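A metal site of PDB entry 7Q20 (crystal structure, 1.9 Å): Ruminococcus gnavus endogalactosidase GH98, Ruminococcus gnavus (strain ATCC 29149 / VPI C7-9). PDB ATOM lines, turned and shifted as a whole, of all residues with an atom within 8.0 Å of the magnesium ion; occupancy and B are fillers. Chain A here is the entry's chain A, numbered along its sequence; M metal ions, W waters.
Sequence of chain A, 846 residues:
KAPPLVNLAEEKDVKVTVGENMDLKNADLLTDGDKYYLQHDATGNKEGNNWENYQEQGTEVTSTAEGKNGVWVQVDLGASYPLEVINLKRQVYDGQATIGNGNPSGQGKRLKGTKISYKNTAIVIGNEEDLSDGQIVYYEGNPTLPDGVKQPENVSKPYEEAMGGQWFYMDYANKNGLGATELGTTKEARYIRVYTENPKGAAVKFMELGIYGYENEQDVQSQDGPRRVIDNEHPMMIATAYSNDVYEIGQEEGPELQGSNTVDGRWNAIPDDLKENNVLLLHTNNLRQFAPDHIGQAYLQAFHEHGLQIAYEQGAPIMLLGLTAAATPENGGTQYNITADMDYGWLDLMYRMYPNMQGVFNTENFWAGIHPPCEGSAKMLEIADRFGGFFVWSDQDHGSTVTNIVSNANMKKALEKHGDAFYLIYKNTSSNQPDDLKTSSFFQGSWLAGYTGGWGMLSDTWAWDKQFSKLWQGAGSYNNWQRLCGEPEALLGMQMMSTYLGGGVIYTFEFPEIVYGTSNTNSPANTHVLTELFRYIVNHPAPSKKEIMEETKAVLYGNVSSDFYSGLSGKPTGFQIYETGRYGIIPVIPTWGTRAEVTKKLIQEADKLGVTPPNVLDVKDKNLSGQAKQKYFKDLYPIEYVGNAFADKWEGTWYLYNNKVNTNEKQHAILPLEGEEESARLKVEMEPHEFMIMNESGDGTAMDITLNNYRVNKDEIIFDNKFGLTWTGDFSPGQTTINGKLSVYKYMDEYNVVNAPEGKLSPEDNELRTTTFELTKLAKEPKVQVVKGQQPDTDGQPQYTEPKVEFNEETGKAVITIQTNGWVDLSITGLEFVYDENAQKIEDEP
The magnesium ion is bound by the side-chain carboxylate of Asp 765 (2.0 Å), the side-chain amide oxygen of Gln 799 (2.0 Å), water W2 (2.0 Å), water W1 (2.0 Å) and the side-chain amide oxygen of Asn 766 (2.0 Å).
The side-chain amide oxygen of Gln 799 lies close to the backbone carbonyl oxygen of Gln 797, 3.5 Å away. The backbone carbonyl oxygen (O) of Asp 765 is in hydrogen-bond range of the side-chain amide nitrogen (ND2) of Asn 821, 3.0 Å away. OD2 of Asp 795 lies within hydrogen-bond range of ND2 of Asn 766, at 3.1 Å. OD2 of Asp 765 is in hydrogen-bond range of OH of Tyr 710 (2.8 Å). O of Gln 799 is in hydrogen-bond range of N of Asn 821 (2.8 Å).
Water W2 lies within hydrogen-bond range of OD2 of Asp 795 (2.6 Å), O of Pro 763 (3.1 Å) and ND2 of Asn 766 (3.3 Å). Water W1 lies within hydrogen-bond range of OD1 of Asp 795 (2.7 Å), O of Gln 797 (2.8 Å) and N of Asp 793 (2.9 Å).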
ATOM      1  N   HIS A 528       9.879 -21.655 -27.868  1.00  0.00           N
ATOM      2  CA  HIS A 528      11.125 -21.396 -27.137  1.00  0.00           C
ATOM      3  C   HIS A 528      12.391 -21.337 -27.999  1.00  0.00           C
ATOM      4  O   HIS A 528      13.436 -20.907 -27.506  1.00  0.00           O
ATOM      5  CB  HIS A 528      11.296 -22.404 -25.976  1.00  0.00           C
ATOM      6  CG  HIS A 528      10.169 -22.382 -24.976  1.00  0.00           C
ATOM      7  ND1 HIS A 528       9.746 -21.237 -24.348  1.00  0.00           N
ATOM      8  CD2 HIS A 528       9.378 -23.383 -24.507  1.00  0.00           C
ATOM      9  CE1 HIS A 528       8.735 -21.522 -23.525  1.00  0.00           C
ATOM     10  NE2 HIS A 528       8.501 -22.823 -23.607  1.00  0.00           N
ATOM     11  N   TYR A 710      17.525 -25.019 -25.396  1.00  0.00           N
ATOM     12  CA  TYR A 710      16.226 -25.664 -25.104  1.00  0.00           C
ATOM     13  C   TYR A 710      16.221 -27.071 -25.701  1.00  0.00           C
ATOM     14  O   TYR A 710      16.478 -27.230 -26.918  1.00  0.00           O
ATOM     15  CB  TYR A 710      15.041 -24.867 -25.661  1.00  0.00           C
ATOM     16  CG  TYR A 710      13.730 -25.397 -25.154  1.00  0.00           C
ATOM     17  CD1 TYR A 710      13.441 -25.397 -23.809  1.00  0.00           C
ATOM     18  CD2 TYR A 710      12.793 -25.950 -26.019  1.00  0.00           C
ATOM     19  CE1 TYR A 710      12.239 -25.902 -23.317  1.00  0.00           C
ATOM     20  CE2 TYR A 710      11.595 -26.449 -25.548  1.00  0.00           C
ATOM     21  CZ  TYR A 710      11.314 -26.426 -24.200  1.00  0.00           C
ATOM     22  OH  TYR A 710      10.132 -26.924 -23.717  1.00  0.00           O
ATOM     23  N   SER A 762       3.225 -30.386 -18.715  1.00  0.00           N
ATOM     24  CA  SER A 762       4.264 -29.464 -19.133  1.00  0.00           C
ATOM     25  C   SER A 762       5.359 -30.264 -19.841  1.00  0.00           C
ATOM     26  O   SER A 762       5.561 -31.444 -19.552  1.00  0.00           O
ATOM     27  CB  SER A 762       4.878 -28.738 -17.922  1.00  0.00           C
ATOM     28  OG  SER A 762       3.889 -28.015 -17.211  1.00  0.00           O
ATOM     29  N   PRO A 763       6.128 -29.659 -20.771  1.00  0.00           N
ATOM     30  CA  PRO A 763       7.207 -30.375 -21.452  1.00  0.00           C
ATOM     31  C   PRO A 763       8.297 -30.844 -20.471  1.00  0.00           C
ATOM     32  O   PRO A 763       8.571 -30.124 -19.508  1.00  0.00           O
ATOM     33  CB  PRO A 763       7.771 -29.334 -22.437  1.00  0.00           C
ATOM     34  CG  PRO A 763       6.639 -28.330 -22.597  1.00  0.00           C
ATOM     35  CD  PRO A 763       5.989 -28.268 -21.235  1.00  0.00           C
ATOM     36  N   GLU A 764       8.860 -32.033 -20.715  1.00  0.00           N
ATOM     37  CA  GLU A 764       9.984 -32.568 -19.950  1.00  0.00           C
ATOM     38  C   GLU A 764      11.281 -31.838 -20.283  1.00  0.00           C
ATOM     39  O   GLU A 764      12.130 -32.365 -21.003  1.00  0.00           O
ATOM     40  CB  GLU A 764      10.136 -34.072 -20.227  1.00  0.00           C
ATOM     41  CG  GLU A 764       9.139 -34.935 -19.475  1.00  0.00           C
ATOM     42  CD  GLU A 764       9.483 -35.094 -17.995  1.00  0.00           C
ATOM     43  OE1 GLU A 764      10.500 -34.536 -17.530  1.00  0.00           O
ATOM     44  OE2 GLU A 764       8.719 -35.792 -17.288  1.00  0.00           O
ATOM     45  N   ASP A 765      11.418 -30.628 -19.734  1.00  0.00           N
ATOM     46  CA  ASP A 765      12.477 -29.703 -20.097  1.00  0.00           C
ATOM     47  C   ASP A 765      13.216 -29.090 -18.885  1.00  0.00           C
ATOM     48  O   ASP A 765      13.902 -28.069 -19.040  1.00  0.00           O
ATOM     49  CB  ASP A 765      11.876 -28.602 -20.974  1.00  0.00           C
ATOM     50  CG  ASP A 765      10.852 -27.734 -20.237  1.00  0.00           C
ATOM     51  OD1 ASP A 765      10.779 -27.787 -18.984  1.00  0.00           O
ATOM     52  OD2 ASP A 765      10.111 -26.990 -20.919  1.00  0.00           O
ATOM     53  N   ASN A 766      13.079 -29.719 -17.720  1.00  0.00           N
ATOM     54  CA  ASN A 766      13.507 -29.138 -16.445  1.00  0.00           C
ATOM     55  C   ASN A 766      14.907 -29.556 -15.954  1.00  0.00           C
ATOM     56  O   ASN A 766      15.437 -28.964 -14.995  1.00  0.00           O
ATOM     57  CB  ASN A 766      12.451 -29.425 -15.365  1.00  0.00           C
ATOM     58  CG  ASN A 766      11.089 -28.867 -15.726  1.00  0.00           C
ATOM     59  OD1 ASN A 766      10.973 -27.761 -16.264  1.00  0.00           O
ATOM     60  ND2 ASN A 766      10.028 -29.618 -15.416  1.00  0.00           N
ATOM     61  N   GLU A 767      15.509 -30.569 -16.602  1.00  0.00           N
ATOM     62  CA  GLU A 767      16.928 -30.897 -16.411  1.00  0.00           C
ATOM     63  C   GLU A 767      17.806 -29.827 -17.102  1.00  0.00           C
ATOM     64  O   GLU A 767      17.745 -29.648 -18.328  1.00  0.00           O
ATOM     65  CB  GLU A 767      17.251 -32.284 -16.959  1.00  0.00           C
ATOM     66  CG  GLU A 767      18.735 -32.675 -16.829  1.00  0.00           C
ATOM     67  CD  GLU A 767      18.963 -34.184 -16.777  1.00  0.00           C
ATOM     68  OE1 GLU A 767      18.202 -34.952 -17.430  1.00  0.00           O
ATOM     69  OE2 GLU A 767      19.926 -34.611 -16.079  1.00  0.00           O
ATOM     70  N   LEU A 768      18.599 -29.122 -16.284  1.00  0.00           N
ATOM     71  CA  LEU A 768      19.446 -28.012 -16.742  1.00  0.00           C
ATOM     72  C   LEU A 768      20.856 -28.503 -17.027  1.00  0.00           C
ATOM     73  O   LEU A 768      21.324 -29.476 -16.437  1.00  0.00           O
ATOM     74  CB  LEU A 768      19.482 -26.898 -15.703  1.00  0.00           C
ATOM     75  CG  LEU A 768      18.128 -26.453 -15.122  1.00  0.00           C
ATOM     76  CD1 LEU A 768      18.334 -25.322 -14.125  1.00  0.00           C
ATOM     77  CD2 LEU A 768      17.139 -26.011 -16.215  1.00  0.00           C
ATOM     78  N   GLN A 790      13.850 -17.306 -19.970  1.00  0.00           N
ATOM     79  CA  GLN A 790      12.706 -18.174 -20.196  1.00  0.00           C
ATOM     80  C   GLN A 790      12.030 -18.509 -18.863  1.00  0.00           C
ATOM     81  O   GLN A 790      12.696 -18.953 -17.926  1.00  0.00           O
ATOM     82  CB  GLN A 790      13.139 -19.447 -20.901  1.00  0.00           C
ATOM     83  CG  GLN A 790      11.971 -20.370 -21.235  1.00  0.00           C
ATOM     84  CD  GLN A 790      12.357 -21.468 -22.184  1.00  0.00           C
ATOM     85  OE1 GLN A 790      13.232 -21.303 -23.029  1.00  0.00           O
ATOM     86  NE2 GLN A 790      11.701 -22.614 -22.052  1.00  0.00           N
ATOM     87  N   GLN A 791      10.711 -18.310 -18.804  1.00  0.00           N
ATOM     88  CA  GLN A 791       9.919 -18.438 -17.579  1.00  0.00           C
ATOM     89  C   GLN A 791       9.439 -19.878 -17.389  1.00  0.00           C
ATOM     90  O   GLN A 791       9.454 -20.656 -18.341  1.00  0.00           O
ATOM     91  CB  GLN A 791       8.732 -17.477 -17.628  1.00  0.00           C
ATOM     92  CG  GLN A 791       9.142 -16.007 -17.631  1.00  0.00           C
ATOM     93  CD  GLN A 791       9.948 -15.617 -16.395  1.00  0.00           C
ATOM     94  OE1 GLN A 791      11.162 -15.381 -16.474  1.00  0.00           O
ATOM     95  NE2 GLN A 791       9.278 -15.571 -15.252  1.00  0.00           N
ATOM     96  N   PRO A 792       9.036 -20.287 -16.170  1.00  0.00           N
ATOM     97  CA  PRO A 792       8.592 -21.663 -15.937  1.00  0.00           C
ATOM     98  C   PRO A 792       7.339 -22.045 -16.743  1.00  0.00           C
ATOM     99  O   PRO A 792       6.593 -21.148 -17.094  1.00  0.00           O
ATOM    100  CB  PRO A 792       8.249 -21.674 -14.439  1.00  0.00           C
ATOM    101  CG  PRO A 792       9.075 -20.556 -13.868  1.00  0.00           C
ATOM    102  CD  PRO A 792       9.020 -19.482 -14.942  1.00  0.00           C
ATOM    103  N   ASP A 793       7.127 -23.339 -17.003  1.00  0.00           N
ATOM    104  CA  ASP A 793       5.813 -23.804 -17.455  1.00  0.00           C
ATOM    105  C   ASP A 793       4.909 -23.852 -16.209  1.00  0.00           C
ATOM    106  O   ASP A 793       5.311 -23.401 -15.131  1.00  0.00           O
ATOM    107  CB  ASP A 793       5.904 -25.154 -18.167  1.00  0.00           C
ATOM    108  CG  ASP A 793       4.789 -25.344 -19.193  1.00  0.00           C
ATOM    109  OD1 ASP A 793       3.691 -25.837 -18.804  1.00  0.00           O
ATOM    110  OD2 ASP A 793       5.015 -25.019 -20.368  1.00  0.00           O
ATOM    111  N   THR A 794       3.691 -24.366 -16.352  1.00  0.00           N
ATOM    112  CA  THR A 794       2.696 -24.400 -15.270  1.00  0.00           C
ATOM    113  C   THR A 794       3.067 -25.302 -14.086  1.00  0.00           C
ATOM    114  O   THR A 794       2.436 -25.229 -13.047  1.00  0.00           O
ATOM    115  CB  THR A 794       1.309 -24.832 -15.813  1.00  0.00           C
ATOM    116  OG1 THR A 794       1.441 -26.027 -16.582  1.00  0.00           O
ATOM    117  CG2 THR A 794       0.697 -23.738 -16.675  1.00  0.00           C
ATOM    118  N   ASP A 795       4.103 -26.147 -14.250  1.00  0.00           N
ATOM    119  CA  ASP A 795       4.596 -26.999 -13.166  1.00  0.00           C
ATOM    120  C   ASP A 795       5.540 -26.253 -12.206  1.00  0.00           C
ATOM    121  O   ASP A 795       6.003 -26.818 -11.235  1.00  0.00           O
ATOM    122  CB  ASP A 795       5.269 -28.270 -13.724  1.00  0.00           C
ATOM    123  CG  ASP A 795       6.531 -27.922 -14.718  1.00  0.00           C
ATOM    124  OD1 ASP A 795       7.103 -26.767 -14.643  1.00  0.00           O
ATOM    125  OD2 ASP A 795       7.076 -28.814 -15.405  1.00  0.00           O
ATOM    126  N   GLY A 796       5.825 -24.984 -12.497  1.00  0.00           N
ATOM    127  CA  GLY A 796       6.584 -24.125 -11.607  1.00  0.00           C
ATOM    128  C   GLY A 796       8.110 -24.292 -11.593  1.00  0.00           C
ATOM    129  O   GLY A 796       8.787 -23.550 -10.894  1.00  0.00           O
ATOM    130  N   GLN A 797       8.627 -25.252 -12.384  1.00  0.00           N
ATOM    131  CA  GLN A 797      10.063 -25.560 -12.382  1.00  0.00           C
ATOM    132  C   GLN A 797      10.854 -24.545 -13.214  1.00  0.00           C
ATOM    133  O   GLN A 797      10.426 -24.183 -14.319  1.00  0.00           O
ATOM    134  CB  GLN A 797      10.343 -26.982 -12.886  1.00  0.00           C
ATOM    135  CG  GLN A 797       9.540 -28.088 -12.223  1.00  0.00           C
ATOM    136  CD  GLN A 797       9.600 -28.025 -10.715  1.00  0.00           C
ATOM    137  OE1 GLN A 797       8.632 -27.637 -10.052  1.00  0.00           O
ATOM    138  NE2 GLN A 797      10.739 -28.398 -10.155  1.00  0.00           N
ATOM    139  N   PRO A 798      12.011 -24.064 -12.709  1.00  0.00           N
ATOM    140  CA  PRO A 798      12.793 -23.043 -13.400  1.00  0.00           C
ATOM    141  C   PRO A 798      13.541 -23.554 -14.648  1.00  0.00           C
ATOM    142  O   PRO A 798      13.938 -24.730 -14.663  1.00  0.00           O
ATOM    143  CB  PRO A 798      13.800 -22.587 -12.317  1.00  0.00           C
ATOM    144  CG  PRO A 798      13.977 -23.811 -11.448  1.00  0.00           C
ATOM    145  CD  PRO A 798      12.617 -24.480 -11.435  1.00  0.00           C
ATOM    146  N   GLN A 799      13.738 -22.653 -15.632  1.00  0.00           N
ATOM    147  CA  GLN A 799      14.447 -22.989 -16.853  1.00  0.00           C
ATOM    148  C   GLN A 799      15.898 -22.480 -16.848  1.00  0.00           C
ATOM    149  O   GLN A 799      16.679 -22.788 -17.754  1.00  0.00           O
ATOM    150  CB  GLN A 799      13.688 -22.449 -18.076  1.00  0.00           C
ATOM    151  CG  GLN A 799      12.258 -22.974 -18.206  1.00  0.00           C
ATOM    152  CD  GLN A 799      12.153 -24.522 -18.176  1.00  0.00           C
ATOM    153  OE1 GLN A 799      11.233 -25.093 -17.563  1.00  0.00           O
ATOM    154  NE2 GLN A 799      13.082 -25.193 -18.866  1.00  0.00           N
ATOM    155  N   ASN A 821      18.020 -24.624 -19.352  1.00  0.00           N
ATOM    156  CA  ASN A 821      17.404 -25.385 -20.423  1.00  0.00           C
ATOM    157  C   ASN A 821      16.370 -24.481 -21.059  1.00  0.00           C
ATOM    158  O   ASN A 821      15.207 -24.461 -20.653  1.00  0.00           O
ATOM    159  CB  ASN A 821      16.765 -26.690 -19.931  1.00  0.00           C
ATOM    160  CG  ASN A 821      16.295 -27.561 -21.079  1.00  0.00           C
ATOM    161  OD1 ASN A 821      16.089 -27.072 -22.175  1.00  0.00           O
ATOM    162  ND2 ASN A 821      16.140 -28.855 -20.837  1.00  0.00           N
HETATM  163 MG    MG M   1       9.918 -26.616 -17.594  1.00  0.00          MG
HETATM  164  O   HOH W   1       8.842 -25.493 -16.264  1.00  0.00           O
HETATM  165  O   HOH W   2       8.263 -27.792 -17.527  1.00  0.00           O
